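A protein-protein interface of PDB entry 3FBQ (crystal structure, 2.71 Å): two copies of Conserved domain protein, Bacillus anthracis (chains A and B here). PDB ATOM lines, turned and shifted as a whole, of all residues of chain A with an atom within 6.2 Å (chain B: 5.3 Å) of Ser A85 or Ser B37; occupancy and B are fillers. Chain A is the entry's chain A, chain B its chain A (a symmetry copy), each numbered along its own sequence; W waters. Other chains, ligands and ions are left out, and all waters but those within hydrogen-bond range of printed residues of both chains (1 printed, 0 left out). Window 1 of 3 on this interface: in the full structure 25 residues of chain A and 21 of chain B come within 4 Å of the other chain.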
ATOM      1  N   GLY A  83      -1.012  16.260   1.785  1.00  0.00           N
ATOM      2  CA  GLY A  83       0.165  17.146   2.012  1.00  0.00           C
ATOM      3  C   GLY A  83      -0.354  18.480   2.471  1.00  0.00           C
ATOM      4  O   GLY A  83      -1.565  18.674   2.618  1.00  0.00           O
ATOM      5  N   SER A  84       0.524  19.439   2.657  1.00  0.00           N
ATOM      6  CA  SER A  84       0.034  20.808   2.734  1.00  0.00           C
ATOM      7  C   SER A  84       1.074  21.807   2.315  1.00  0.00           C
ATOM      8  O   SER A  84       2.274  21.564   2.524  1.00  0.00           O
ATOM      9  CB  SER A  84      -0.453  21.131   4.130  1.00  0.00           C
ATOM     10  OG  SER A  84       0.623  21.576   4.907  1.00  0.00           O
ATOM     11  N   SER A  85       0.618  22.913   1.717  1.00  0.00           N
ATOM     12  CA  SER A  85       1.467  24.081   1.527  1.00  0.00           C
ATOM     13  C   SER A  85       0.884  25.387   2.063  1.00  0.00           C
ATOM     14  O   SER A  85      -0.263  25.431   2.496  1.00  0.00           O
ATOM     15  CB  SER A  85       1.947  24.195   0.085  1.00  0.00           C
ATOM     16  OG  SER A  85       0.941  24.290  -0.894  1.00  0.00           O
ATOM     17  N   GLY A  86       1.666  26.458   2.093  1.00  0.00           N
ATOM     18  CA  GLY A  86       1.157  27.686   2.690  1.00  0.00           C
ATOM     19  C   GLY A  86       2.056  28.860   2.471  1.00  0.00           C
ATOM     20  O   GLY A  86       3.103  28.734   1.856  1.00  0.00           O
ATOM     21  N   SER A  87       1.635  29.994   3.003  1.00  0.00           N
ATOM     22  CA  SER A  87       2.269  31.285   2.885  1.00  0.00           C
ATOM     23  C   SER A  87       1.901  32.115   4.099  1.00  0.00           C
ATOM     24  O   SER A  87       0.886  31.861   4.758  1.00  0.00           O
ATOM     25  CB  SER A  87       1.653  31.988   1.698  1.00  0.00           C
ATOM     26  OG  SER A  87       2.553  32.082   0.598  1.00  0.00           O
ATOM     27  N   THR A 103      -1.995  31.361   5.379  1.00  0.00           N
ATOM     28  CA  THR A 103      -2.705  30.674   4.332  1.00  0.00           C
ATOM     29  C   THR A 103      -2.256  29.226   4.349  1.00  0.00           C
ATOM     30  O   THR A 103      -1.082  28.996   4.254  1.00  0.00           O
ATOM     31  CB  THR A 103      -2.154  31.282   3.032  1.00  0.00           C
ATOM     32  OG1 THR A 103      -2.943  32.405   2.724  1.00  0.00           O
ATOM     33  CG2 THR A 103      -2.111  30.343   1.848  1.00  0.00           C
ATOM     34  N   THR A 104      -3.137  28.237   4.421  1.00  0.00           N
ATOM     35  CA  THR A 104      -2.676  26.853   4.212  1.00  0.00           C
ATOM     36  C   THR A 104      -3.511  26.089   3.153  1.00  0.00           C
ATOM     37  O   THR A 104      -4.733  26.187   3.131  1.00  0.00           O
ATOM     38  CB  THR A 104      -2.618  26.112   5.535  1.00  0.00           C
ATOM     39  OG1 THR A 104      -1.950  26.952   6.471  1.00  0.00           O
ATOM     40  CG2 THR A 104      -1.856  24.802   5.410  1.00  0.00           C
ATOM     41  N   THR A 105      -2.842  25.352   2.279  1.00  0.00           N
ATOM     42  CA  THR A 105      -3.504  24.598   1.247  1.00  0.00           C
ATOM     43  C   THR A 105      -3.263  23.110   1.482  1.00  0.00           C
ATOM     44  O   THR A 105      -2.109  22.672   1.513  1.00  0.00           O
ATOM     45  CB  THR A 105      -2.994  25.049  -0.148  1.00  0.00           C
ATOM     46  OG1 THR A 105      -3.279  26.441  -0.232  1.00  0.00           O
ATOM     47  CG2 THR A 105      -3.752  24.406  -1.244  1.00  0.00           C
ATOM     48  N   HIS A 106      -4.325  22.335   1.644  1.00  0.00           N
ATOM     49  CA  HIS A 106      -4.147  20.921   1.815  1.00  0.00           C
ATOM     50  C   HIS A 106      -4.109  20.231   0.399  1.00  0.00           C
ATOM     51  O   HIS A 106      -4.497  20.866  -0.589  1.00  0.00           O
ATOM     52  CB  HIS A 106      -5.244  20.407   2.707  1.00  0.00           C
ATOM     53  CG  HIS A 106      -6.524  20.166   1.979  1.00  0.00           C
ATOM     54  ND1 HIS A 106      -7.548  21.082   1.947  1.00  0.00           N
ATOM     55  CD2 HIS A 106      -6.939  19.114   1.237  1.00  0.00           C
ATOM     56  CE1 HIS A 106      -8.546  20.604   1.232  1.00  0.00           C
ATOM     57  NE2 HIS A 106      -8.207  19.405   0.796  1.00  0.00           N
ATOM     58  N   HIS A 107      -3.578  19.005   0.289  1.00  0.00           N
ATOM     59  CA  HIS A 107      -3.531  18.256  -0.997  1.00  0.00           C
ATOM     60  C   HIS A 107      -4.226  16.902  -0.874  1.00  0.00           C
ATOM     61  O   HIS A 107      -3.838  15.881  -1.430  1.00  0.00           O
ATOM     62  CB  HIS A 107      -2.109  18.104  -1.520  1.00  0.00           C
ATOM     63  CG  HIS A 107      -1.368  19.387  -1.543  1.00  0.00           C
ATOM     64  ND1 HIS A 107      -0.122  19.549  -0.958  1.00  0.00           N
ATOM     65  CD2 HIS A 107      -1.723  20.603  -2.023  1.00  0.00           C
ATOM     66  CE1 HIS A 107       0.274  20.798  -1.118  1.00  0.00           C
ATOM     67  NE2 HIS A 107      -0.695  21.463  -1.734  1.00  0.00           N
ATOM     68  N   ASN A 214      -0.784  28.396  -4.876  1.00  0.00           N
ATOM     69  CA  ASN A 214      -1.099  27.785  -3.588  1.00  0.00           C
ATOM     70  C   ASN A 214      -0.135  26.687  -3.307  1.00  0.00           C
ATOM     71  O   ASN A 214      -0.339  25.953  -2.339  1.00  0.00           O
ATOM     72  CB  ASN A 214      -2.476  27.130  -3.592  1.00  0.00           C
ATOM     73  CG  ASN A 214      -3.541  28.045  -4.107  1.00  0.00           C
ATOM     74  OD1 ASN A 214      -3.524  29.259  -3.827  1.00  0.00           O
ATOM     75  ND2 ASN A 214      -4.497  27.476  -4.876  1.00  0.00           N
ATOM     76  N   GLY A 215       0.871  26.537  -4.176  1.00  0.00           N
ATOM     77  CA  GLY A 215       1.924  25.562  -3.994  1.00  0.00           C
ATOM     78  C   GLY A 215       1.898  24.468  -5.038  1.00  0.00           C
ATOM     79  O   GLY A 215       0.848  24.188  -5.619  1.00  0.00           O
ATOM     80  N   GLY A 216       3.057  23.836  -5.253  1.00  0.00           N
ATOM     81  CA  GLY A 216       3.204  22.676  -6.119  1.00  0.00           C
ATOM     82  C   GLY A 216       3.888  21.487  -5.465  1.00  0.00           C
ATOM     83  O   GLY A 216       4.538  21.601  -4.419  1.00  0.00           O
ATOM     84  N   ARG B  35       8.656  19.917  -3.201  1.00  0.00           N
ATOM     85  CA  ARG B  35       7.619  20.769  -2.655  1.00  0.00           C
ATOM     86  C   ARG B  35       7.921  22.236  -2.923  1.00  0.00           C
ATOM     87  O   ARG B  35       9.045  22.678  -2.728  1.00  0.00           O
ATOM     88  CB  ARG B  35       7.502  20.560  -1.145  1.00  0.00           C
ATOM     89  CG  ARG B  35       6.269  19.742  -0.729  1.00  0.00           C
ATOM     90  CD  ARG B  35       6.078  18.581  -1.668  1.00  0.00           C
ATOM     91  NE  ARG B  35       5.709  17.363  -0.974  1.00  0.00           N
ATOM     92  CZ  ARG B  35       5.722  16.149  -1.509  1.00  0.00           C
ATOM     93  NH1 ARG B  35       6.114  15.939  -2.769  1.00  0.00           N
ATOM     94  NH2 ARG B  35       5.332  15.141  -0.754  1.00  0.00           N
ATOM     95  N   GLU B  36       6.930  22.997  -3.388  1.00  0.00           N
ATOM     96  CA  GLU B  36       7.156  24.425  -3.635  1.00  0.00           C
ATOM     97  C   GLU B  36       6.109  25.450  -3.193  1.00  0.00           C
ATOM     98  O   GLU B  36       5.023  25.462  -3.736  1.00  0.00           O
ATOM     99  CB  GLU B  36       7.432  24.654  -5.107  1.00  0.00           C
ATOM    100  CG  GLU B  36       8.291  25.869  -5.232  1.00  0.00           C
ATOM    101  CD  GLU B  36       8.530  26.277  -6.617  1.00  0.00           C
ATOM    102  OE1 GLU B  36       8.446  27.503  -6.847  1.00  0.00           O
ATOM    103  OE2 GLU B  36       8.801  25.394  -7.466  1.00  0.00           O
ATOM    104  N   SER B  37       6.451  26.339  -2.261  1.00  0.00           N
ATOM    105  CA  SER B  37       5.583  27.464  -1.879  1.00  0.00           C
ATOM    106  C   SER B  37       6.465  28.687  -1.779  1.00  0.00           C
ATOM    107  O   SER B  37       7.668  28.562  -1.545  1.00  0.00           O
ATOM    108  CB  SER B  37       4.902  27.264  -0.518  1.00  0.00           C
ATOM    109  OG  SER B  37       4.509  25.941  -0.257  1.00  0.00           O
ATOM    110  N   ASN B  38       5.873  29.858  -1.975  1.00  0.00           N
ATOM    111  CA  ASN B  38       6.496  31.120  -1.643  1.00  0.00           C
ATOM    112  C   ASN B  38       7.819  31.446  -2.205  1.00  0.00           C
ATOM    113  O   ASN B  38       8.629  32.056  -1.502  1.00  0.00           O
ATOM    114  CB  ASN B  38       6.732  31.208  -0.174  1.00  0.00           C
ATOM    115  CG  ASN B  38       5.645  31.880   0.519  1.00  0.00           C
ATOM    116  OD1 ASN B  38       4.758  31.191   1.048  1.00  0.00           O
ATOM    117  ND2 ASN B  38       5.643  33.234   0.511  1.00  0.00           N
ATOM    118  N   GLY B  39       8.056  31.076  -3.441  1.00  0.00           N
ATOM    119  CA  GLY B  39       9.346  31.282  -4.033  1.00  0.00           C
ATOM    120  C   GLY B  39      10.409  30.278  -3.638  1.00  0.00           C
ATOM    121  O   GLY B  39      11.550  30.390  -4.113  1.00  0.00           O
ATOM    122  N   VAL B  40      10.060  29.298  -2.790  1.00  0.00           N
ATOM    123  CA  VAL B  40      11.019  28.318  -2.318  1.00  0.00           C
ATOM    124  C   VAL B  40      10.684  26.828  -2.698  1.00  0.00           C
ATOM    125  O   VAL B  40       9.704  26.226  -2.236  1.00  0.00           O
ATOM    126  CB  VAL B  40      11.218  28.499  -0.742  1.00  0.00           C
ATOM    127  CG1 VAL B  40      12.357  27.621  -0.167  1.00  0.00           C
ATOM    128  CG2 VAL B  40      11.444  29.965  -0.401  1.00  0.00           C
ATOM    129  N   LYS B  41      11.562  26.235  -3.496  1.00  0.00           N
ATOM    130  CA  LYS B  41      11.457  24.860  -3.918  1.00  0.00           C
ATOM    131  C   LYS B  41      12.349  24.054  -3.024  1.00  0.00           C
ATOM    132  O   LYS B  41      13.562  24.277  -3.044  1.00  0.00           O
ATOM    133  CB  LYS B  41      11.955  24.794  -5.374  1.00  0.00           C
ATOM    134  CG  LYS B  41      11.546  23.538  -6.143  1.00  0.00           C
ATOM    135  CD  LYS B  41      11.876  23.566  -7.634  1.00  0.00           C
ATOM    136  CE  LYS B  41      11.713  22.140  -8.179  1.00  0.00           C
ATOM    137  NZ  LYS B  41      12.337  21.808  -9.519  1.00  0.00           N
ATOM    138  N   HIS B 136       4.629  26.329   4.409  1.00  0.00           N
ATOM    139  CA  HIS B 136       4.668  24.908   4.703  1.00  0.00           C
ATOM    140  C   HIS B 136       5.328  24.135   3.551  1.00  0.00           C
ATOM    141  O   HIS B 136       4.927  24.274   2.391  1.00  0.00           O
ATOM    142  CB  HIS B 136       3.239  24.406   4.821  1.00  0.00           C
ATOM    143  CG  HIS B 136       2.712  24.427   6.206  1.00  0.00           C
ATOM    144  ND1 HIS B 136       1.436  24.872   6.514  1.00  0.00           N
ATOM    145  CD2 HIS B 136       3.283  24.075   7.381  1.00  0.00           C
ATOM    146  CE1 HIS B 136       1.230  24.749   7.809  1.00  0.00           C
ATOM    147  NE2 HIS B 136       2.337  24.274   8.362  1.00  0.00           N
ATOM    148  N   TRP B 137       6.260  23.262   3.851  1.00  0.00           N
ATOM    149  CA  TRP B 137       6.777  22.378   2.846  1.00  0.00           C
ATOM    150  C   TRP B 137       6.869  21.088   3.587  1.00  0.00           C
ATOM    151  O   TRP B 137       7.541  21.037   4.589  1.00  0.00           O
ATOM    152  CB  TRP B 137       8.163  22.822   2.442  1.00  0.00           C
ATOM    153  CG  TRP B 137       8.286  24.218   1.802  1.00  0.00           C
ATOM    154  CD1 TRP B 137       8.445  24.481   0.493  1.00  0.00           C
ATOM    155  CD2 TRP B 137       8.285  25.516   2.476  1.00  0.00           C
ATOM    156  NE1 TRP B 137       8.524  25.854   0.277  1.00  0.00           N
ATOM    157  CE2 TRP B 137       8.439  26.504   1.476  1.00  0.00           C
ATOM    158  CE3 TRP B 137       8.130  25.926   3.814  1.00  0.00           C
ATOM    159  CZ2 TRP B 137       8.468  27.876   1.774  1.00  0.00           C
ATOM    160  CZ3 TRP B 137       8.158  27.267   4.110  1.00  0.00           C
ATOM    161  CH2 TRP B 137       8.325  28.237   3.105  1.00  0.00           C
ATOM    162  N   ASN B 138       6.162  20.054   3.154  1.00  0.00           N
ATOM    163  CA  ASN B 138       6.012  18.828   3.927  1.00  0.00           C
ATOM    164  C   ASN B 138       6.308  17.615   3.092  1.00  0.00           C
ATOM    165  O   ASN B 138       5.897  17.559   1.933  1.00  0.00           O
ATOM    166  CB  ASN B 138       4.589  18.718   4.451  1.00  0.00           C
ATOM    167  CG  ASN B 138       4.191  19.924   5.279  1.00  0.00           C
ATOM    168  OD1 ASN B 138       3.023  20.276   5.319  1.00  0.00           O
ATOM    169  ND2 ASN B 138       5.173  20.621   5.886  1.00  0.00           N
HETATM  170  O   HOH W   1       4.230  20.689   0.945  1.00  0.00           O
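Printed residues of chain A that touch a printed residue of chain B: Ser A84, Ser A85, Gly A86, Ser A87, Thr A104, Gly A215 and Gly A216.
Among the printed residues, no Asp or Glu carboxylate lies within 4 Å of a Lys or Arg side-chain nitrogen of the other chain.
His A106 touches none of the printed residues of chain B.
Of the printed residues of chain A, Arg B35 touches Gly A216.
Ser B37 touches just these residues of chain A: Ser A85 and Gly A86.
Printed residues of chain A within 4 Å of Asn B38: Gly A86 and Ser A87.
Gly B39 touches none of the printed residues of chain A.
Of the printed residues of chain A, His B136 touches Ser A84 (3.8 Å), Ser A85 (3.6 Å), Gly A86 (3.8 Å) and Thr A104 (3.5 Å).
The nearest printed residue of chain B that does not touch Ser A85 is Glu B36 (5.1 Å).
The nearest residue of chain A that does not touch Ser B37 is Gly A215 (4.6 Å).
The nearest printed residue of chain A that does not touch Asn B138 is Gly A83 (4.8 Å).
No position is printed for both chains.
Water W1 lies within hydrogen-bond range of the backbone carbonyl oxygen of Ser A84 (2.7 Å) and the backbone NH of Asn B138 (3.0 Å).
ND1 of His B136 touches OG of Ser A84, 3.8 Å away.
Ser A85 touches Ser B37.
Ser A85 touches His B136.
O of Gly A86 touches CB of Ser B37 (3.3 Å).
His B136 touches Gly A86 (CB to N, 3.8 Å).
ND1 of His B136 touches CG2 of Thr A104 (3.5 Å).
CA of Gly A215 touches O of Glu B36, at 3.1 Å.
Gly A216 touches Arg B35 (O to CA, 3.6 Å).
The backbone carbonyl oxygen (O) of Ser A85 lies within hydrogen-bond range of the backbone NH (N) of Thr A105 (2.6 Å).
OG of Ser A85 lies within hydrogen-bond range of NE2 of His A107, 3.4 Å away.
O of Asn A214 lies within hydrogen-bond range of OG of Ser A85 (2.5 Å).
O of Ser A87 is in hydrogen-bond range of N of Thr A103.
The guanidinium group (NE) of Arg B35 lies within hydrogen-bond range of the backbone carbonyl oxygen (O) of Asn B138, at 2.9 Å.
The side-chain hydroxyl (OG) of Ser B37 lies within hydrogen-bond range of the backbone carbonyl oxygen (O) of His B136 (3.2 Å).
The side-chain hydroxyl of Ser A84 sits at hydrogen-bond distance from the side-chain amide oxygen of Asn B138, 2.8 Å away.
The backbone carbonyl oxygen (O) of Gly A86 sits close to the side-chain amide oxygen (OD1) of Asn B38, 3.1 Å away.
The side-chain hydroxyl (OG) of Ser A87 lies within hydrogen-bond range of the side-chain amide oxygen (OD1) of Asn B38.
The backbone NH of Glu B36 lies within hydrogen-bond range of the backbone carbonyl oxygen of Gly A216 (3.0 Å).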
